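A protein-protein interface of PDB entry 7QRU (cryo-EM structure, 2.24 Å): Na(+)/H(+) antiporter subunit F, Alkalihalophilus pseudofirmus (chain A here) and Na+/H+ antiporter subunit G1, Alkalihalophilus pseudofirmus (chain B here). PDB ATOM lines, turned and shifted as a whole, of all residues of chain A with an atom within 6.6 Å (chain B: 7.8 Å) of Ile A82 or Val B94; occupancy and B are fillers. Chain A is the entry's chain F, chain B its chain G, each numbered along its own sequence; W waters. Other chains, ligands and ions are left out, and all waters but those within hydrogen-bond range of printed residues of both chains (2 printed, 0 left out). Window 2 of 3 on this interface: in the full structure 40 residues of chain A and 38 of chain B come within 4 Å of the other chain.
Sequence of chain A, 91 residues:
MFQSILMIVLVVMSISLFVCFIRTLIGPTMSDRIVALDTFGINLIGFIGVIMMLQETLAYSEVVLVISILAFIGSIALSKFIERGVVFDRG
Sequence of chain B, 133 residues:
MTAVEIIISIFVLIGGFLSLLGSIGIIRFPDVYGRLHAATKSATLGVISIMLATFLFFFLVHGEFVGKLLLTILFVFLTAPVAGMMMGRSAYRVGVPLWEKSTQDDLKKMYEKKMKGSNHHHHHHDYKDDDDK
The side-chain carboxylate (OE2) of Glu A83 is in salt-bridge range of the guanidinium group (NE) of Arg A84.
The backbone NH of Val B96 lies within hydrogen-bond range of the backbone carbonyl oxygen of Ala B91.
Met A30 touches none of the printed residues of chain B.
Printed residues of chain B within 4 Å of Ser A31: Ala B91.
Of the printed residues of chain B, Ser A79 touches Met B87 and Ser B90.
Phe A81 touches none of the printed residues of chain B.
Of chain B, only Ser B90 (3.7 Å) and Val B94 (3.4 Å) come within 4 Å of Ile A82.
Of the printed residues of chain A, Ser B90 touches Ser A79, Ile A82 and Glu A83.
Of chain A, only Ile A82 comes within 4 Å of Val B94.
The nearest printed residue of chain A that does not touch Arg B93 is Arg A84 (5.0 Å).
The side-chain hydroxyl of Ser B90 lies within hydrogen-bond range of the backbone carbonyl oxygen of Ser A79 (2.7 Å).
The side-chain carboxylate (OE2) of Glu A83 lies within salt-bridge range of the guanidinium group (NH1) of Arg B93, 3.0 Å away.
The backbone carbonyl oxygen of Ile A34 sits close to the side-chain sulfur of Met B87, 3.8 Å away.
Ser A31 touches Ala B91 (OG to CB, 3.3 Å).
Met B87 touches Ser A79.
CG2 of Ile A82 touches OG of Ser B90, 3.7 Å away.
Ile A82 touches Val B94.
Ser B90 touches Glu A83 (OG to CB, 3.7 Å).
Water W1 lies within hydrogen-bond range of OG of Ser A31 (2.8 Å), O of Met B87 (2.9 Å), OG of Ser B90 (3.1 Å) and N of Ala B91 (3.4 Å).
Water W2 bridges the side-chain carboxylate (OE1) of Glu A83 (3.0 Å) and the backbone NH (N) of Ser B90 (3.4 Å).
Of the 14 printed residues of chain A, 5 touch a printed residue of chain B.
Printed residues of chain B that touch a printed residue of chain A: Met B87, Ser B90, Ala B91, Arg B93 and Val B94.
Hydrophobic or aromatic side chains of chain B that line the printed part of chain A: Met B87, Ala B91 and Val B94.
Among the printed residues, 8 pairs touch across the chains.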
ATOM      1  N   MET A  30      -5.138  -2.745 -11.657  1.00  0.00           N
ATOM      2  CA  MET A  30      -5.329  -4.134 -11.992  1.00  0.00           C
ATOM      3  C   MET A  30      -6.254  -4.839 -11.028  1.00  0.00           C
ATOM      4  O   MET A  30      -7.023  -5.644 -11.513  1.00  0.00           O
ATOM      5  CB  MET A  30      -4.038  -4.919 -12.016  1.00  0.00           C
ATOM      6  CG  MET A  30      -3.199  -4.650 -13.216  1.00  0.00           C
ATOM      7  SD  MET A  30      -3.954  -4.551 -14.883  1.00  0.00           S
ATOM      8  CE  MET A  30      -3.020  -3.214 -15.580  1.00  0.00           C
ATOM      9  N   SER A  31      -6.267  -4.496  -9.748  1.00  0.00           N
ATOM     10  CA  SER A  31      -7.180  -5.139  -8.819  1.00  0.00           C
ATOM     11  C   SER A  31      -8.591  -4.869  -9.273  1.00  0.00           C
ATOM     12  O   SER A  31      -9.400  -5.779  -9.250  1.00  0.00           O
ATOM     13  CB  SER A  31      -6.860  -4.649  -7.421  1.00  0.00           C
ATOM     14  OG  SER A  31      -5.601  -5.226  -7.064  1.00  0.00           O
ATOM     15  N   ASP A  32      -8.895  -3.601  -9.630  1.00  0.00           N
ATOM     16  CA  ASP A  32     -10.196  -3.214 -10.113  1.00  0.00           C
ATOM     17  C   ASP A  32     -10.639  -4.078 -11.319  1.00  0.00           C
ATOM     18  O   ASP A  32     -11.776  -4.483 -11.435  1.00  0.00           O
ATOM     19  CB  ASP A  32     -10.188  -1.761 -10.542  1.00  0.00           C
ATOM     20  CG  ASP A  32     -10.450  -0.806  -9.401  1.00  0.00           C
ATOM     21  OD1 ASP A  32     -11.616  -0.872  -8.862  1.00  0.00           O
ATOM     22  OD2 ASP A  32      -9.538   0.078  -9.096  1.00  0.00           O
ATOM     23  N   ILE A  34      -9.714  -7.172 -12.106  1.00  0.00           N
ATOM     24  CA  ILE A  34      -9.984  -8.556 -11.779  1.00  0.00           C
ATOM     25  C   ILE A  34     -11.285  -8.623 -10.971  1.00  0.00           C
ATOM     26  O   ILE A  34     -11.975  -9.643 -11.058  1.00  0.00           O
ATOM     27  CB  ILE A  34      -8.808  -9.269 -11.080  1.00  0.00           C
ATOM     28  CG1 ILE A  34      -8.570  -8.744  -9.670  1.00  0.00           C
ATOM     29  CG2 ILE A  34      -7.539  -9.124 -11.882  1.00  0.00           C
ATOM     30  CD1 ILE A  34      -7.692  -9.609  -8.900  1.00  0.00           C
ATOM     31  N   ALA A  77      -6.148 -17.073  -9.190  1.00  0.00           N
ATOM     32  CA  ALA A  77      -4.940 -16.997  -9.972  1.00  0.00           C
ATOM     33  C   ALA A  77      -4.538 -15.576 -10.343  1.00  0.00           C
ATOM     34  O   ALA A  77      -3.382 -15.185 -10.126  1.00  0.00           O
ATOM     35  CB  ALA A  77      -5.098 -17.800 -11.203  1.00  0.00           C
ATOM     36  N   LEU A  78      -5.458 -14.737 -10.767  1.00  0.00           N
ATOM     37  CA  LEU A  78      -5.103 -13.367 -11.112  1.00  0.00           C
ATOM     38  C   LEU A  78      -4.790 -12.552  -9.871  1.00  0.00           C
ATOM     39  O   LEU A  78      -3.935 -11.707  -9.884  1.00  0.00           O
ATOM     40  CB  LEU A  78      -6.226 -12.734 -11.889  1.00  0.00           C
ATOM     41  CG  LEU A  78      -6.392 -13.218 -13.309  1.00  0.00           C
ATOM     42  CD1 LEU A  78      -7.771 -12.801 -13.839  1.00  0.00           C
ATOM     43  CD2 LEU A  78      -5.347 -12.601 -14.131  1.00  0.00           C
ATOM     44  N   SER A  79      -5.403 -12.808  -8.768  1.00  0.00           N
ATOM     45  CA  SER A  79      -5.067 -12.128  -7.532  1.00  0.00           C
ATOM     46  C   SER A  79      -3.658 -12.428  -7.078  1.00  0.00           C
ATOM     47  O   SER A  79      -2.989 -11.569  -6.541  1.00  0.00           O
ATOM     48  CB  SER A  79      -6.002 -12.615  -6.416  1.00  0.00           C
ATOM     49  OG  SER A  79      -7.168 -11.857  -6.547  1.00  0.00           O
ATOM     50  N   LYS A  80      -3.246 -13.688  -7.191  1.00  0.00           N
ATOM     51  CA  LYS A  80      -1.920 -14.078  -6.789  1.00  0.00           C
ATOM     52  C   LYS A  80      -0.868 -13.541  -7.766  1.00  0.00           C
ATOM     53  O   LYS A  80       0.172 -13.078  -7.368  1.00  0.00           O
ATOM     54  CB  LYS A  80      -1.781 -15.594  -6.770  1.00  0.00           C
ATOM     55  CG  LYS A  80      -2.631 -16.333  -5.796  1.00  0.00           C
ATOM     56  CD  LYS A  80      -2.283 -17.815  -5.767  1.00  0.00           C
ATOM     57  CE  LYS A  80      -0.809 -18.044  -5.495  1.00  0.00           C
ATOM     58  NZ  LYS A  80      -0.647 -19.492  -5.191  1.00  0.00           N
ATOM     59  N   PHE A  81      -1.180 -13.579  -9.068  1.00  0.00           N
ATOM     60  CA  PHE A  81      -0.267 -13.030 -10.040  1.00  0.00           C
ATOM     61  C   PHE A  81       0.045 -11.593  -9.674  1.00  0.00           C
ATOM     62  O   PHE A  81       1.190 -11.167  -9.789  1.00  0.00           O
ATOM     63  CB  PHE A  81      -0.836 -13.168 -11.473  1.00  0.00           C
ATOM     64  CG  PHE A  81       0.230 -12.919 -12.492  1.00  0.00           C
ATOM     65  CD1 PHE A  81       1.348 -13.788 -12.623  1.00  0.00           C
ATOM     66  CD2 PHE A  81       0.247 -11.669 -13.105  1.00  0.00           C
ATOM     67  CE1 PHE A  81       2.350 -13.434 -13.516  1.00  0.00           C
ATOM     68  CE2 PHE A  81       1.317 -11.306 -13.916  1.00  0.00           C
ATOM     69  CZ  PHE A  81       2.344 -12.201 -14.141  1.00  0.00           C
ATOM     70  N   ILE A  82      -1.006 -10.781  -9.484  1.00  0.00           N
ATOM     71  CA  ILE A  82      -0.861  -9.368  -9.209  1.00  0.00           C
ATOM     72  C   ILE A  82       0.018  -9.169  -7.965  1.00  0.00           C
ATOM     73  O   ILE A  82       0.861  -8.287  -7.980  1.00  0.00           O
ATOM     74  CB  ILE A  82      -2.238  -8.733  -9.067  1.00  0.00           C
ATOM     75  CG1 ILE A  82      -2.833  -8.551 -10.444  1.00  0.00           C
ATOM     76  CG2 ILE A  82      -2.291  -7.435  -8.277  1.00  0.00           C
ATOM     77  CD1 ILE A  82      -4.419  -8.222 -10.201  1.00  0.00           C
ATOM     78  N   GLU A  83      -0.174  -9.955  -6.931  1.00  0.00           N
ATOM     79  CA  GLU A  83       0.516  -9.756  -5.670  1.00  0.00           C
ATOM     80  C   GLU A  83       1.954 -10.316  -5.714  1.00  0.00           C
ATOM     81  O   GLU A  83       2.864  -9.744  -5.149  1.00  0.00           O
ATOM     82  CB  GLU A  83      -0.362 -10.339  -4.553  1.00  0.00           C
ATOM     83  CG  GLU A  83       0.378 -10.796  -3.338  1.00  0.00           C
ATOM     84  CD  GLU A  83      -0.296 -11.827  -2.437  1.00  0.00           C
ATOM     85  OE1 GLU A  83      -1.513 -12.094  -2.583  1.00  0.00           O
ATOM     86  OE2 GLU A  83       0.442 -12.399  -1.589  1.00  0.00           O
ATOM     87  N   ARG A  84       2.186 -11.453  -6.308  1.00  0.00           N
ATOM     88  CA  ARG A  84       3.459 -12.156  -6.218  1.00  0.00           C
ATOM     89  C   ARG A  84       4.154 -12.332  -7.585  1.00  0.00           C
ATOM     90  O   ARG A  84       5.382 -12.471  -7.604  1.00  0.00           O
ATOM     91  CB  ARG A  84       3.224 -13.550  -5.625  1.00  0.00           C
ATOM     92  CG  ARG A  84       3.371 -13.569  -4.128  1.00  0.00           C
ATOM     93  CD  ARG A  84       2.888 -14.883  -3.532  1.00  0.00           C
ATOM     94  NE  ARG A  84       1.467 -14.747  -3.292  1.00  0.00           N
ATOM     95  CZ  ARG A  84       0.690 -15.691  -2.784  1.00  0.00           C
ATOM     96  NH1 ARG A  84       1.226 -16.820  -2.352  1.00  0.00           N
ATOM     97  NH2 ARG A  84      -0.628 -15.565  -2.873  1.00  0.00           N
ATOM     98  N   GLY A  85       3.405 -12.330  -8.683  1.00  0.00           N
ATOM     99  CA  GLY A  85       3.972 -12.566  -9.968  1.00  0.00           C
ATOM    100  C   GLY A  85       4.182 -14.043 -10.248  1.00  0.00           C
ATOM    101  O   GLY A  85       4.706 -14.326 -11.306  1.00  0.00           O
ATOM    102  N   VAL A  86       3.706 -14.939  -9.369  1.00  0.00           N
ATOM    103  CA  VAL A  86       3.710 -16.375  -9.651  1.00  0.00           C
ATOM    104  C   VAL A  86       2.294 -16.903  -9.430  1.00  0.00           C
ATOM    105  O   VAL A  86       1.736 -16.718  -8.374  1.00  0.00           O
ATOM    106  CB  VAL A  86       4.722 -17.138  -8.774  1.00  0.00           C
ATOM    107  CG1 VAL A  86       6.132 -17.042  -9.298  1.00  0.00           C
ATOM    108  CG2 VAL A  86       4.714 -16.636  -7.360  1.00  0.00           C
ATOM    109  N   TYR B  33     -11.832  -1.454  -2.590  1.00  0.00           N
ATOM    110  CA  TYR B  33     -12.335  -2.125  -1.376  1.00  0.00           C
ATOM    111  C   TYR B  33     -13.855  -2.003  -1.244  1.00  0.00           C
ATOM    112  O   TYR B  33     -14.474  -3.001  -0.966  1.00  0.00           O
ATOM    113  CB  TYR B  33     -11.684  -1.546  -0.138  1.00  0.00           C
ATOM    114  CG  TYR B  33     -10.188  -1.609  -0.290  1.00  0.00           C
ATOM    115  CD1 TYR B  33      -9.543  -2.831  -0.228  1.00  0.00           C
ATOM    116  CD2 TYR B  33      -9.436  -0.465  -0.583  1.00  0.00           C
ATOM    117  CE1 TYR B  33      -8.205  -2.959  -0.565  1.00  0.00           C
ATOM    118  CE2 TYR B  33      -8.107  -0.591  -0.913  1.00  0.00           C
ATOM    119  CZ  TYR B  33      -7.467  -1.816  -0.767  1.00  0.00           C
ATOM    120  OH  TYR B  33      -6.138  -1.845  -1.088  1.00  0.00           O
ATOM    121  N   MET B  87      -8.942 -11.113  -3.566  1.00  0.00           N
ATOM    122  CA  MET B  87      -8.874  -9.885  -4.347  1.00  0.00           C
ATOM    123  C   MET B  87      -8.668  -8.639  -3.479  1.00  0.00           C
ATOM    124  O   MET B  87      -7.984  -7.753  -3.890  1.00  0.00           O
ATOM    125  CB  MET B  87     -10.093  -9.675  -5.301  1.00  0.00           C
ATOM    126  CG  MET B  87     -10.141 -10.806  -6.327  1.00  0.00           C
ATOM    127  SD  MET B  87     -11.573 -10.818  -7.479  1.00  0.00           S
ATOM    128  CE  MET B  87     -12.946 -10.621  -6.346  1.00  0.00           C
ATOM    129  N   GLY B  88      -9.175  -8.535  -2.304  1.00  0.00           N
ATOM    130  CA  GLY B  88      -8.962  -7.311  -1.598  1.00  0.00           C
ATOM    131  C   GLY B  88      -7.625  -7.322  -0.943  1.00  0.00           C
ATOM    132  O   GLY B  88      -7.008  -6.275  -0.894  1.00  0.00           O
ATOM    133  N   ARG B  89      -7.163  -8.515  -0.484  1.00  0.00           N
ATOM    134  CA  ARG B  89      -5.900  -8.572   0.231  1.00  0.00           C
ATOM    135  C   ARG B  89      -4.749  -8.471  -0.770  1.00  0.00           C
ATOM    136  O   ARG B  89      -3.802  -7.852  -0.506  1.00  0.00           O
ATOM    137  CB  ARG B  89      -5.762  -9.867   0.957  1.00  0.00           C
ATOM    138  CG  ARG B  89      -4.511  -9.916   1.827  1.00  0.00           C
ATOM    139  CD  ARG B  89      -4.693 -11.061   2.775  1.00  0.00           C
ATOM    140  NE  ARG B  89      -4.501 -12.210   1.944  1.00  0.00           N
ATOM    141  CZ  ARG B  89      -4.527 -13.418   2.445  1.00  0.00           C
ATOM    142  NH1 ARG B  89      -4.909 -13.585   3.713  1.00  0.00           N
ATOM    143  NH2 ARG B  89      -4.156 -14.418   1.671  1.00  0.00           N
ATOM    144  N   SER B  90      -4.873  -9.048  -1.948  1.00  0.00           N
ATOM    145  CA  SER B  90      -3.918  -8.869  -2.987  1.00  0.00           C
ATOM    146  C   SER B  90      -3.747  -7.393  -3.349  1.00  0.00           C
ATOM    147  O   SER B  90      -2.628  -6.940  -3.509  1.00  0.00           O
ATOM    148  CB  SER B  90      -4.376  -9.684  -4.248  1.00  0.00           C
ATOM    149  OG  SER B  90      -3.742  -9.229  -5.425  1.00  0.00           O
ATOM    150  N   ALA B  91      -4.849  -6.640  -3.469  1.00  0.00           N
ATOM    151  CA  ALA B  91      -4.799  -5.209  -3.745  1.00  0.00           C
ATOM    152  C   ALA B  91      -4.051  -4.478  -2.665  1.00  0.00           C
ATOM    153  O   ALA B  91      -3.239  -3.622  -2.960  1.00  0.00           O
ATOM    154  CB  ALA B  91      -6.164  -4.649  -3.823  1.00  0.00           C
ATOM    155  N   TYR B  92      -4.350  -4.821  -1.393  1.00  0.00           N
ATOM    156  CA  TYR B  92      -3.750  -4.060  -0.278  1.00  0.00           C
ATOM    157  C   TYR B  92      -2.223  -4.343  -0.257  1.00  0.00           C
ATOM    158  O   TYR B  92      -1.443  -3.448  -0.038  1.00  0.00           O
ATOM    159  CB  TYR B  92      -4.466  -4.400   1.033  1.00  0.00           C
ATOM    160  CG  TYR B  92      -4.094  -3.481   2.174  1.00  0.00           C
ATOM    161  CD1 TYR B  92      -2.995  -3.697   2.981  1.00  0.00           C
ATOM    162  CD2 TYR B  92      -4.798  -2.353   2.396  1.00  0.00           C
ATOM    163  CE1 TYR B  92      -2.617  -2.816   3.948  1.00  0.00           C
ATOM    164  CE2 TYR B  92      -4.479  -1.468   3.398  1.00  0.00           C
ATOM    165  CZ  TYR B  92      -3.371  -1.696   4.174  1.00  0.00           C
ATOM    166  OH  TYR B  92      -3.041  -0.834   5.182  1.00  0.00           O
ATOM    167  N   ARG B  93      -1.810  -5.592  -0.474  1.00  0.00           N
ATOM    168  CA  ARG B  93      -0.435  -5.908  -0.454  1.00  0.00           C
ATOM    169  C   ARG B  93       0.287  -5.238  -1.644  1.00  0.00           C
ATOM    170  O   ARG B  93       1.430  -4.861  -1.537  1.00  0.00           O
ATOM    171  CB  ARG B  93      -0.276  -7.429  -0.480  1.00  0.00           C
ATOM    172  CG  ARG B  93      -0.672  -8.161   0.786  1.00  0.00           C
ATOM    173  CD  ARG B  93      -0.613  -9.599   0.644  1.00  0.00           C
ATOM    174  NE  ARG B  93      -0.878 -10.290   1.882  1.00  0.00           N
ATOM    175  CZ  ARG B  93      -1.070 -11.607   2.018  1.00  0.00           C
ATOM    176  NH1 ARG B  93      -1.148 -12.399   0.965  1.00  0.00           N
ATOM    177  NH2 ARG B  93      -1.266 -12.108   3.223  1.00  0.00           N
ATOM    178  N   VAL B  94      -0.329  -5.170  -2.800  1.00  0.00           N
ATOM    179  CA  VAL B  94       0.308  -4.627  -4.003  1.00  0.00           C
ATOM    180  C   VAL B  94       0.395  -3.090  -3.905  1.00  0.00           C
ATOM    181  O   VAL B  94       1.073  -2.468  -4.680  1.00  0.00           O
ATOM    182  CB  VAL B  94      -0.417  -5.115  -5.282  1.00  0.00           C
ATOM    183  CG1 VAL B  94      -1.502  -4.185  -5.711  1.00  0.00           C
ATOM    184  CG2 VAL B  94       0.578  -5.347  -6.356  1.00  0.00           C
ATOM    185  N   GLY B  95      -0.248  -2.526  -2.903  1.00  0.00           N
ATOM    186  CA  GLY B  95      -0.166  -1.132  -2.596  1.00  0.00           C
ATOM    187  C   GLY B  95      -1.354  -0.300  -3.051  1.00  0.00           C
ATOM    188  O   GLY B  95      -1.254   0.952  -2.995  1.00  0.00           O
ATOM    189  N   VAL B  96      -2.408  -0.914  -3.605  1.00  0.00           N
ATOM    190  CA  VAL B  96      -3.584  -0.107  -3.976  1.00  0.00           C
ATOM    191  C   VAL B  96      -4.087   0.628  -2.736  1.00  0.00           C
ATOM    192  O   VAL B  96      -4.281  -0.038  -1.722  1.00  0.00           O
ATOM    193  CB  VAL B  96      -4.700  -0.951  -4.597  1.00  0.00           C
ATOM    194  CG1 VAL B  96      -5.897  -0.114  -4.745  1.00  0.00           C
ATOM    195  CG2 VAL B  96      -4.214  -1.628  -5.878  1.00  0.00           C
ATOM    196  N   PRO B  97      -4.119   1.984  -2.663  1.00  0.00           N
ATOM    197  CA  PRO B  97      -4.410   2.696  -1.420  1.00  0.00           C
ATOM    198  C   PRO B  97      -5.891   2.661  -1.114  1.00  0.00           C
ATOM    199  O   PRO B  97      -6.761   2.621  -2.020  1.00  0.00           O
ATOM    200  CB  PRO B  97      -4.147   4.182  -1.755  1.00  0.00           C
ATOM    201  CG  PRO B  97      -3.418   4.128  -3.033  1.00  0.00           C
ATOM    202  CD  PRO B  97      -3.954   2.939  -3.749  1.00  0.00           C
HETATM  203  O   HOH W   1      -6.374  -7.809  -6.308  1.00  0.00           O
HETATM  204  O   HOH W   2      -4.431 -12.392  -1.750  1.00  0.00           O
